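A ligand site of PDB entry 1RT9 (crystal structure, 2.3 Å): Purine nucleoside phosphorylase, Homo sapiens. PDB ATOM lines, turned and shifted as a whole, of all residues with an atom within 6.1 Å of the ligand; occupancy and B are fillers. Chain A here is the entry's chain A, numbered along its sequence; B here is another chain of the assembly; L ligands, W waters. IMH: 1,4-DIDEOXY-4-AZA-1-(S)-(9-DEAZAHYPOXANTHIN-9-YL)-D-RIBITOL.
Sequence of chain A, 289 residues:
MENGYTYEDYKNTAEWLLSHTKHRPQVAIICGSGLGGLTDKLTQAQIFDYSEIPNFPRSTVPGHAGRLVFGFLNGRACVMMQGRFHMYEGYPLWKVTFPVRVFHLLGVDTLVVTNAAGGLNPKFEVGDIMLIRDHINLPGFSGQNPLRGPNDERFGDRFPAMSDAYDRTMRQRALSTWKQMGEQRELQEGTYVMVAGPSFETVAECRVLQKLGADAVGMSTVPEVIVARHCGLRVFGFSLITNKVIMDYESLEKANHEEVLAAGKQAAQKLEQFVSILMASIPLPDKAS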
ATOM      1  N   SER A  33      30.021   7.852   0.420  1.00  0.00           N
ATOM      2  CA  SER A  33      28.932   8.822   0.370  1.00  0.00           C
ATOM      3  C   SER A  33      29.150  10.008   1.316  1.00  0.00           C
ATOM      4  O   SER A  33      29.351   9.816   2.529  1.00  0.00           O
ATOM      5  CB  SER A  33      27.606   8.128   0.697  1.00  0.00           C
ATOM      6  OG  SER A  33      26.550   9.059   0.782  1.00  0.00           O
ATOM      7  N   HIS A  86      28.204   1.201  -7.706  1.00  0.00           N
ATOM      8  CA  HIS A  86      27.522   0.266  -6.836  1.00  0.00           C
ATOM      9  C   HIS A  86      26.811  -0.838  -7.612  1.00  0.00           C
ATOM     10  O   HIS A  86      26.357  -0.638  -8.731  1.00  0.00           O
ATOM     11  CB  HIS A  86      26.474   0.969  -5.956  1.00  0.00           C
ATOM     12  CG  HIS A  86      27.022   2.079  -5.137  1.00  0.00           C
ATOM     13  ND1 HIS A  86      27.129   3.377  -5.600  1.00  0.00           N
ATOM     14  CD2 HIS A  86      27.492   2.102  -3.871  1.00  0.00           C
ATOM     15  CE1 HIS A  86      27.644   4.138  -4.664  1.00  0.00           C
ATOM     16  NE2 HIS A  86      27.875   3.393  -3.599  1.00  0.00           N
ATOM     17  N   TYR A  88      23.978  -2.168  -6.685  1.00  0.00           N
ATOM     18  CA  TYR A  88      22.557  -1.847  -6.723  1.00  0.00           C
ATOM     19  C   TYR A  88      22.129  -0.954  -7.884  1.00  0.00           C
ATOM     20  O   TYR A  88      20.937  -0.879  -8.207  1.00  0.00           O
ATOM     21  CB  TYR A  88      22.088  -1.236  -5.377  1.00  0.00           C
ATOM     22  CG  TYR A  88      22.717   0.093  -4.980  1.00  0.00           C
ATOM     23  CD1 TYR A  88      22.458   1.260  -5.704  1.00  0.00           C
ATOM     24  CD2 TYR A  88      23.545   0.168  -3.871  1.00  0.00           C
ATOM     25  CE1 TYR A  88      23.018   2.491  -5.321  1.00  0.00           C
ATOM     26  CE2 TYR A  88      24.115   1.388  -3.470  1.00  0.00           C
ATOM     27  CZ  TYR A  88      23.838   2.533  -4.198  1.00  0.00           C
ATOM     28  OH  TYR A  88      24.392   3.718  -3.782  1.00  0.00           O
ATOM     29  N   ASN A 115      33.233   4.651   3.450  1.00  0.00           N
ATOM     30  CA  ASN A 115      31.842   4.518   3.086  1.00  0.00           C
ATOM     31  C   ASN A 115      30.989   4.974   4.249  1.00  0.00           C
ATOM     32  O   ASN A 115      31.501   5.277   5.315  1.00  0.00           O
ATOM     33  CB  ASN A 115      31.499   3.045   2.765  1.00  0.00           C
ATOM     34  CG  ASN A 115      31.699   2.112   3.962  1.00  0.00           C
ATOM     35  OD1 ASN A 115      31.171   2.361   5.049  1.00  0.00           O
ATOM     36  ND2 ASN A 115      32.449   1.035   3.754  1.00  0.00           N
ATOM     37  N   ALA A 116      29.684   5.063   4.021  1.00  0.00           N
ATOM     38  CA  ALA A 116      28.751   5.438   5.060  1.00  0.00           C
ATOM     39  C   ALA A 116      28.054   4.121   5.374  1.00  0.00           C
ATOM     40  O   ALA A 116      27.867   3.297   4.476  1.00  0.00           O
ATOM     41  CB  ALA A 116      27.753   6.445   4.520  1.00  0.00           C
ATOM     42  N   ALA A 117      27.684   3.902   6.628  1.00  0.00           N
ATOM     43  CA  ALA A 117      27.041   2.647   6.972  1.00  0.00           C
ATOM     44  C   ALA A 117      26.155   2.743   8.199  1.00  0.00           C
ATOM     45  O   ALA A 117      26.316   3.625   9.036  1.00  0.00           O
ATOM     46  CB  ALA A 117      28.099   1.569   7.167  1.00  0.00           C
ATOM     47  N   GLY A 118      25.206   1.831   8.295  1.00  0.00           N
ATOM     48  CA  GLY A 118      24.331   1.828   9.447  1.00  0.00           C
ATOM     49  C   GLY A 118      25.079   1.139  10.566  1.00  0.00           C
ATOM     50  O   GLY A 118      25.900   0.248  10.327  1.00  0.00           O
ATOM     51  N   GLY A 119      24.793   1.554  11.799  1.00  0.00           N
ATOM     52  CA  GLY A 119      25.443   0.934  12.931  1.00  0.00           C
ATOM     53  C   GLY A 119      24.598  -0.227  13.381  1.00  0.00           C
ATOM     54  O   GLY A 119      23.396  -0.096  13.534  1.00  0.00           O
ATOM     55  N   TYR A 192      32.480  -5.139   9.033  1.00  0.00           N
ATOM     56  CA  TYR A 192      31.576  -4.514   8.077  1.00  0.00           C
ATOM     57  C   TYR A 192      30.863  -5.589   7.244  1.00  0.00           C
ATOM     58  O   TYR A 192      31.504  -6.454   6.656  1.00  0.00           O
ATOM     59  CB  TYR A 192      32.364  -3.616   7.129  1.00  0.00           C
ATOM     60  CG  TYR A 192      31.552  -2.987   6.021  1.00  0.00           C
ATOM     61  CD1 TYR A 192      30.955  -1.745   6.192  1.00  0.00           C
ATOM     62  CD2 TYR A 192      31.400  -3.634   4.796  1.00  0.00           C
ATOM     63  CE1 TYR A 192      30.237  -1.150   5.168  1.00  0.00           C
ATOM     64  CE2 TYR A 192      30.672  -3.048   3.760  1.00  0.00           C
ATOM     65  CZ  TYR A 192      30.106  -1.807   3.962  1.00  0.00           C
ATOM     66  OH  TYR A 192      29.407  -1.212   2.948  1.00  0.00           O
ATOM     67  N   VAL A 195      25.632  -5.815   1.988  1.00  0.00           N
ATOM     68  CA  VAL A 195      24.364  -6.339   1.480  1.00  0.00           C
ATOM     69  C   VAL A 195      24.217  -5.520   0.204  1.00  0.00           C
ATOM     70  O   VAL A 195      24.763  -4.408   0.112  1.00  0.00           O
ATOM     71  CB  VAL A 195      23.170  -6.056   2.406  1.00  0.00           C
ATOM     72  CG1 VAL A 195      23.327  -6.789   3.726  1.00  0.00           C
ATOM     73  CG2 VAL A 195      23.019  -4.567   2.612  1.00  0.00           C
ATOM     74  N   SER A 199      17.398  -1.068  -1.109  1.00  0.00           N
ATOM     75  CA  SER A 199      16.444  -0.792  -0.035  1.00  0.00           C
ATOM     76  C   SER A 199      17.089  -1.103   1.328  1.00  0.00           C
ATOM     77  O   SER A 199      17.983  -1.946   1.410  1.00  0.00           O
ATOM     78  CB  SER A 199      15.143  -1.592  -0.242  1.00  0.00           C
ATOM     79  OG  SER A 199      15.374  -2.998  -0.274  1.00  0.00           O
ATOM     80  N   PHE A 200      16.627  -0.436   2.389  1.00  0.00           N
ATOM     81  CA  PHE A 200      17.181  -0.649   3.718  1.00  0.00           C
ATOM     82  C   PHE A 200      16.611  -1.863   4.432  1.00  0.00           C
ATOM     83  O   PHE A 200      15.507  -2.330   4.124  1.00  0.00           O
ATOM     84  CB  PHE A 200      16.971   0.594   4.595  1.00  0.00           C
ATOM     85  CG  PHE A 200      17.804   1.779   4.178  1.00  0.00           C
ATOM     86  CD1 PHE A 200      19.191   1.692   4.133  1.00  0.00           C
ATOM     87  CD2 PHE A 200      17.196   2.981   3.827  1.00  0.00           C
ATOM     88  CE1 PHE A 200      19.974   2.776   3.741  1.00  0.00           C
ATOM     89  CE2 PHE A 200      17.967   4.084   3.438  1.00  0.00           C
ATOM     90  CZ  PHE A 200      19.356   3.975   3.399  1.00  0.00           C
ATOM     91  N   GLU A 201      17.380  -2.361   5.399  1.00  0.00           N
ATOM     92  CA  GLU A 201      17.018  -3.551   6.165  1.00  0.00           C
ATOM     93  C   GLU A 201      15.743  -3.454   6.991  1.00  0.00           C
ATOM     94  O   GLU A 201      15.384  -2.389   7.477  1.00  0.00           O
ATOM     95  CB  GLU A 201      18.146  -3.927   7.119  1.00  0.00           C
ATOM     96  CG  GLU A 201      19.514  -4.159   6.494  1.00  0.00           C
ATOM     97  CD  GLU A 201      20.136  -2.882   5.931  1.00  0.00           C
ATOM     98  OE1 GLU A 201      19.794  -1.784   6.412  1.00  0.00           O
ATOM     99  OE2 GLU A 201      20.971  -2.992   5.016  1.00  0.00           O
ATOM    100  N   VAL A 217      26.658  -2.005   8.556  1.00  0.00           N
ATOM    101  CA  VAL A 217      26.152  -2.531   7.293  1.00  0.00           C
ATOM    102  C   VAL A 217      26.140  -1.481   6.194  1.00  0.00           C
ATOM    103  O   VAL A 217      25.677  -0.360   6.385  1.00  0.00           O
ATOM    104  CB  VAL A 217      24.720  -3.079   7.461  1.00  0.00           C
ATOM    105  CG1 VAL A 217      23.773  -1.961   7.859  1.00  0.00           C
ATOM    106  CG2 VAL A 217      24.267  -3.726   6.168  1.00  0.00           C
ATOM    107  N   GLY A 218      26.684  -1.871   5.044  1.00  0.00           N
ATOM    108  CA  GLY A 218      26.718  -0.973   3.910  1.00  0.00           C
ATOM    109  C   GLY A 218      26.415  -1.706   2.612  1.00  0.00           C
ATOM    110  O   GLY A 218      26.193  -2.920   2.604  1.00  0.00           O
ATOM    111  N   MET A 219      26.416  -0.970   1.513  1.00  0.00           N
ATOM    112  CA  MET A 219      26.105  -1.530   0.212  1.00  0.00           C
ATOM    113  C   MET A 219      27.271  -1.445  -0.746  1.00  0.00           C
ATOM    114  O   MET A 219      27.072  -1.467  -1.953  1.00  0.00           O
ATOM    115  CB  MET A 219      24.884  -0.788  -0.348  1.00  0.00           C
ATOM    116  CG  MET A 219      23.582  -1.348   0.171  1.00  0.00           C
ATOM    117  SD  MET A 219      22.226  -0.153   0.321  1.00  0.00           S
ATOM    118  CE  MET A 219      22.260   0.586  -1.162  1.00  0.00           C
ATOM    119  N   SER A 220      28.489  -1.407  -0.224  1.00  0.00           N
ATOM    120  CA  SER A 220      29.659  -1.276  -1.084  1.00  0.00           C
ATOM    121  C   SER A 220      30.949  -1.823  -0.483  1.00  0.00           C
ATOM    122  O   SER A 220      30.934  -2.694   0.372  1.00  0.00           O
ATOM    123  CB  SER A 220      29.885   0.209  -1.367  1.00  0.00           C
ATOM    124  OG  SER A 220      30.257   0.871  -0.151  1.00  0.00           O
ATOM    125  N   THR A 242      26.430   6.730   9.821  1.00  0.00           N
ATOM    126  CA  THR A 242      25.454   7.795   9.572  1.00  0.00           C
ATOM    127  C   THR A 242      24.089   7.529  10.190  1.00  0.00           C
ATOM    128  O   THR A 242      23.205   8.380  10.130  1.00  0.00           O
ATOM    129  CB  THR A 242      25.272   8.016   8.060  1.00  0.00           C
ATOM    130  OG1 THR A 242      24.647   6.849   7.485  1.00  0.00           O
ATOM    131  CG2 THR A 242      26.620   8.260   7.378  1.00  0.00           C
ATOM    132  N   ASN A 243      23.908   6.357  10.775  1.00  0.00           N
ATOM    133  CA  ASN A 243      22.630   6.029  11.392  1.00  0.00           C
ATOM    134  C   ASN A 243      22.682   4.728  12.178  1.00  0.00           C
ATOM    135  O   ASN A 243      23.547   3.889  11.957  1.00  0.00           O
ATOM    136  CB  ASN A 243      21.544   5.921  10.311  1.00  0.00           C
ATOM    137  CG  ASN A 243      21.910   4.934   9.210  1.00  0.00           C
ATOM    138  OD1 ASN A 243      22.796   5.179   8.401  1.00  0.00           O
ATOM    139  ND2 ASN A 243      21.228   3.793   9.197  1.00  0.00           N
ATOM    140  N   VAL A 245      20.690   1.475  12.773  1.00  0.00           N
ATOM    141  CA  VAL A 245      19.612   0.689  12.182  1.00  0.00           C
ATOM    142  C   VAL A 245      18.595   0.336  13.258  1.00  0.00           C
ATOM    143  O   VAL A 245      18.960   0.122  14.406  1.00  0.00           O
ATOM    144  CB  VAL A 245      20.157  -0.589  11.498  1.00  0.00           C
ATOM    145  CG1 VAL A 245      21.273  -0.232  10.523  1.00  0.00           C
ATOM    146  CG2 VAL A 245      20.675  -1.572  12.523  1.00  0.00           C
ATOM    147  N   ALA A 255      15.151   4.724   8.444  1.00  0.00           N
ATOM    148  CA  ALA A 255      16.444   5.085   7.883  1.00  0.00           C
ATOM    149  C   ALA A 255      16.147   5.719   6.517  1.00  0.00           C
ATOM    150  O   ALA A 255      15.400   5.145   5.714  1.00  0.00           O
ATOM    151  CB  ALA A 255      17.314   3.832   7.707  1.00  0.00           C
ATOM    152  N   ASN A 256      16.708   6.887   6.273  1.00  0.00           N
ATOM    153  CA  ASN A 256      16.465   7.572   5.006  1.00  0.00           C
ATOM    154  C   ASN A 256      17.726   8.240   4.484  1.00  0.00           C
ATOM    155  O   ASN A 256      18.589   8.670   5.243  1.00  0.00           O
ATOM    156  CB  ASN A 256      15.348   8.605   5.179  1.00  0.00           C
ATOM    157  CG  ASN A 256      15.536   9.478   6.409  1.00  0.00           C
ATOM    158  OD1 ASN A 256      16.442  10.311   6.463  1.00  0.00           O
ATOM    159  ND2 ASN A 256      14.684   9.277   7.417  1.00  0.00           N
ATOM    160  N   HIS A 257      17.830   8.309   3.157  1.00  0.00           N
ATOM    161  CA  HIS A 257      18.979   8.903   2.513  1.00  0.00           C
ATOM    162  C   HIS A 257      19.234  10.336   3.021  1.00  0.00           C
ATOM    163  O   HIS A 257      20.373  10.782   3.102  1.00  0.00           O
ATOM    164  CB  HIS A 257      18.751   8.896   0.995  1.00  0.00           C
ATOM    165  CG  HIS A 257      19.965   9.277   0.194  1.00  0.00           C
ATOM    166  ND1 HIS A 257      21.185   8.668   0.371  1.00  0.00           N
ATOM    167  CD2 HIS A 257      20.121  10.158  -0.822  1.00  0.00           C
ATOM    168  CE1 HIS A 257      22.044   9.164  -0.499  1.00  0.00           C
ATOM    169  NE2 HIS A 257      21.421  10.069  -1.232  1.00  0.00           N
ATOM    170  N   VAL A 260      21.326  10.189   6.129  1.00  0.00           N
ATOM    171  CA  VAL A 260      22.677   9.710   5.829  1.00  0.00           C
ATOM    172  C   VAL A 260      23.524  10.863   5.306  1.00  0.00           C
ATOM    173  O   VAL A 260      24.643  11.085   5.757  1.00  0.00           O
ATOM    174  CB  VAL A 260      22.665   8.586   4.760  1.00  0.00           C
ATOM    175  CG1 VAL A 260      24.098   8.187   4.401  1.00  0.00           C
ATOM    176  CG2 VAL A 260      21.905   7.374   5.273  1.00  0.00           C
ATOM    177  N   LEU A 261      22.972  11.588   4.342  1.00  0.00           N
ATOM    178  CA  LEU A 261      23.650  12.724   3.747  1.00  0.00           C
ATOM    179  C   LEU A 261      23.911  13.782   4.823  1.00  0.00           C
ATOM    180  O   LEU A 261      24.970  14.411   4.853  1.00  0.00           O
ATOM    181  CB  LEU A 261      22.812  13.321   2.623  1.00  0.00           C
ATOM    182  CG  LEU A 261      22.458  12.387   1.476  1.00  0.00           C
ATOM    183  CD1 LEU A 261      21.505  13.099   0.513  1.00  0.00           C
ATOM    184  CD2 LEU A 261      23.728  11.946   0.757  1.00  0.00           C
ATOM    185  N   PHE B 159      16.660   4.710  -2.142  1.00  0.00           N
ATOM    186  CA  PHE B 159      16.878   3.893  -0.957  1.00  0.00           C
ATOM    187  C   PHE B 159      15.634   3.790  -0.071  1.00  0.00           C
ATOM    188  O   PHE B 159      15.631   4.292   1.061  1.00  0.00           O
ATOM    189  CB  PHE B 159      18.035   4.477  -0.135  1.00  0.00           C
ATOM    190  CG  PHE B 159      19.296   4.699  -0.930  1.00  0.00           C
ATOM    191  CD1 PHE B 159      20.135   3.642  -1.267  1.00  0.00           C
ATOM    192  CD2 PHE B 159      19.655   5.983  -1.327  1.00  0.00           C
ATOM    193  CE1 PHE B 159      21.316   3.854  -1.993  1.00  0.00           C
ATOM    194  CE2 PHE B 159      20.833   6.216  -2.060  1.00  0.00           C
ATOM    195  CZ  PHE B 159      21.664   5.147  -2.388  1.00  0.00           C
HETATM  196  O5' IMH L   1      22.637   6.555   1.573  1.00  0.00           O
HETATM  197  C5' IMH L   1      22.641   5.235   1.040  1.00  0.00           C
HETATM  198  C4' IMH L   1      24.041   4.746   1.032  1.00  0.00           C
HETATM  199  N4' IMH L   1      24.635   4.734   2.341  1.00  0.00           N
HETATM  200  C3' IMH L   1      24.094   3.355   0.467  1.00  0.00           C
HETATM  201  O3' IMH L   1      24.865   3.477  -0.736  1.00  0.00           O
HETATM  202  C2' IMH L   1      24.785   2.540   1.516  1.00  0.00           C
HETATM  203  O2' IMH L   1      25.996   1.981   0.982  1.00  0.00           O
HETATM  204  C1' IMH L   1      25.101   3.436   2.749  1.00  0.00           C
HETATM  205  C9  IMH L   1      24.293   3.086   4.017  1.00  0.00           C
HETATM  206  C8  IMH L   1      24.102   3.942   5.096  1.00  0.00           C
HETATM  207  N7  IMH L   1      23.381   3.465   6.069  1.00  0.00           N
HETATM  208  C5  IMH L   1      23.039   2.180   5.656  1.00  0.00           C
HETATM  209  C6  IMH L   1      22.233   1.192   6.326  1.00  0.00           C
HETATM  210  O6  IMH L   1      21.689   1.307   7.412  1.00  0.00           O
HETATM  211  N1  IMH L   1      22.095  -0.001   5.602  1.00  0.00           N
HETATM  212  C2  IMH L   1      22.674  -0.237   4.344  1.00  0.00           C
HETATM  213  N3  IMH L   1      23.424   0.701   3.697  1.00  0.00           N
HETATM  214  C4  IMH L   1      23.582   1.899   4.402  1.00  0.00           C
HETATM  215  O   HOH W   1      28.757   1.512   2.606  1.00  0.00           O
HETATM  216  O   HOH W   2      18.988   0.674   7.760  1.00  0.00           O
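Water W2 lies within hydrogen-bond range of O6 of the ligand and OE1 of Glu 201.
Water W1 lies within hydrogen-bond range of O of Ala 116 (2.7 Å), OH of Tyr 192 (2.8 Å), OG of Ser 220 (3.2 Å) and O2' of the ligand (3.2 Å).
The side-chain amide oxygen (OD1) of Asn 243 lies within hydrogen-bond range of a nitrogen (N7) of the ligand (3.0 Å).
The side-chain hydroxyl of Tyr 88 is in hydrogen-bond range of an oxygen (O3') of the ligand (3.1 Å).
The side-chain sulfur (SD) of Met 219 lies close to a nitrogen (N3) of the ligand (3.7 Å).
The backbone NH (N) of Gly 118 lies close to a nitrogen (N7) of the ligand.
N of Met 219 sits at hydrogen-bond distance from O2' of the ligand.
A ring nitrogen (ND1) of His 257 is in hydrogen-bond range of an oxygen (O5') of the ligand (2.8 Å).
A nitrogen (N1) of the ligand lies within hydrogen-bond range of the side-chain carboxylate (OE1) of Glu 201.
OH of Tyr 88 lies within hydrogen-bond range of ND1 of His 86.
O of Ala 117 is in hydrogen-bond range of N of Thr 242, 3.2 Å away.
The backbone NH (N) of Val 245 sits at hydrogen-bond distance from the backbone carbonyl oxygen (O) of Gly 119, 3.2 Å away.
The backbone carbonyl oxygen (O) of Gly 218 lies within hydrogen-bond range of the backbone NH (N) of Val 195, 3.0 Å away.
The side-chain hydroxyl (OH) of Tyr 192 lies within hydrogen-bond range of the backbone NH (N) of Met 219, at 3.3 Å.
N of Gly 119 is in hydrogen-bond range of O of Asn 243, at 2.7 Å.
N of Gly 118 sits at hydrogen-bond distance from O of Val 217, 2.9 Å away.
The side-chain amide oxygen of Asn 243 is in hydrogen-bond range of the side-chain hydroxyl of Thr 242 (2.7 Å).
Ala 116 touches the ligand.
Ala 117 touches the ligand (C to N7, 3.6 Å).
Phe 200 touches the ligand (CE1 to C5, 3.7 Å).
Val 217 touches the ligand.
Gly 218 touches the ligand.
OG1 of Thr 242 touches C8 of the ligand, at 3.8 Å.
Val 245 touches the ligand.
Val 260 touches the ligand.
Phe 159 of chain B touches the ligand.
Hydrophobic or aromatic side chains that line the ligand: Tyr 88, Phe 200, Val 217, Met 219, Val 245, His 257, Val 260 and Phe 159 of chain B.
15 residues have an atom within 4 Å of the ligand: Tyr 88, Ala 116, Ala 117, Gly 118, Phe 200, Glu 201, Val 217, Gly 218, Met 219, Thr 242, Asn 243, Val 245, His 257, Val 260 and Phe 159 of chain B.
Along chain A the residues within 4 Å of the ligand span positions 88 to 260.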
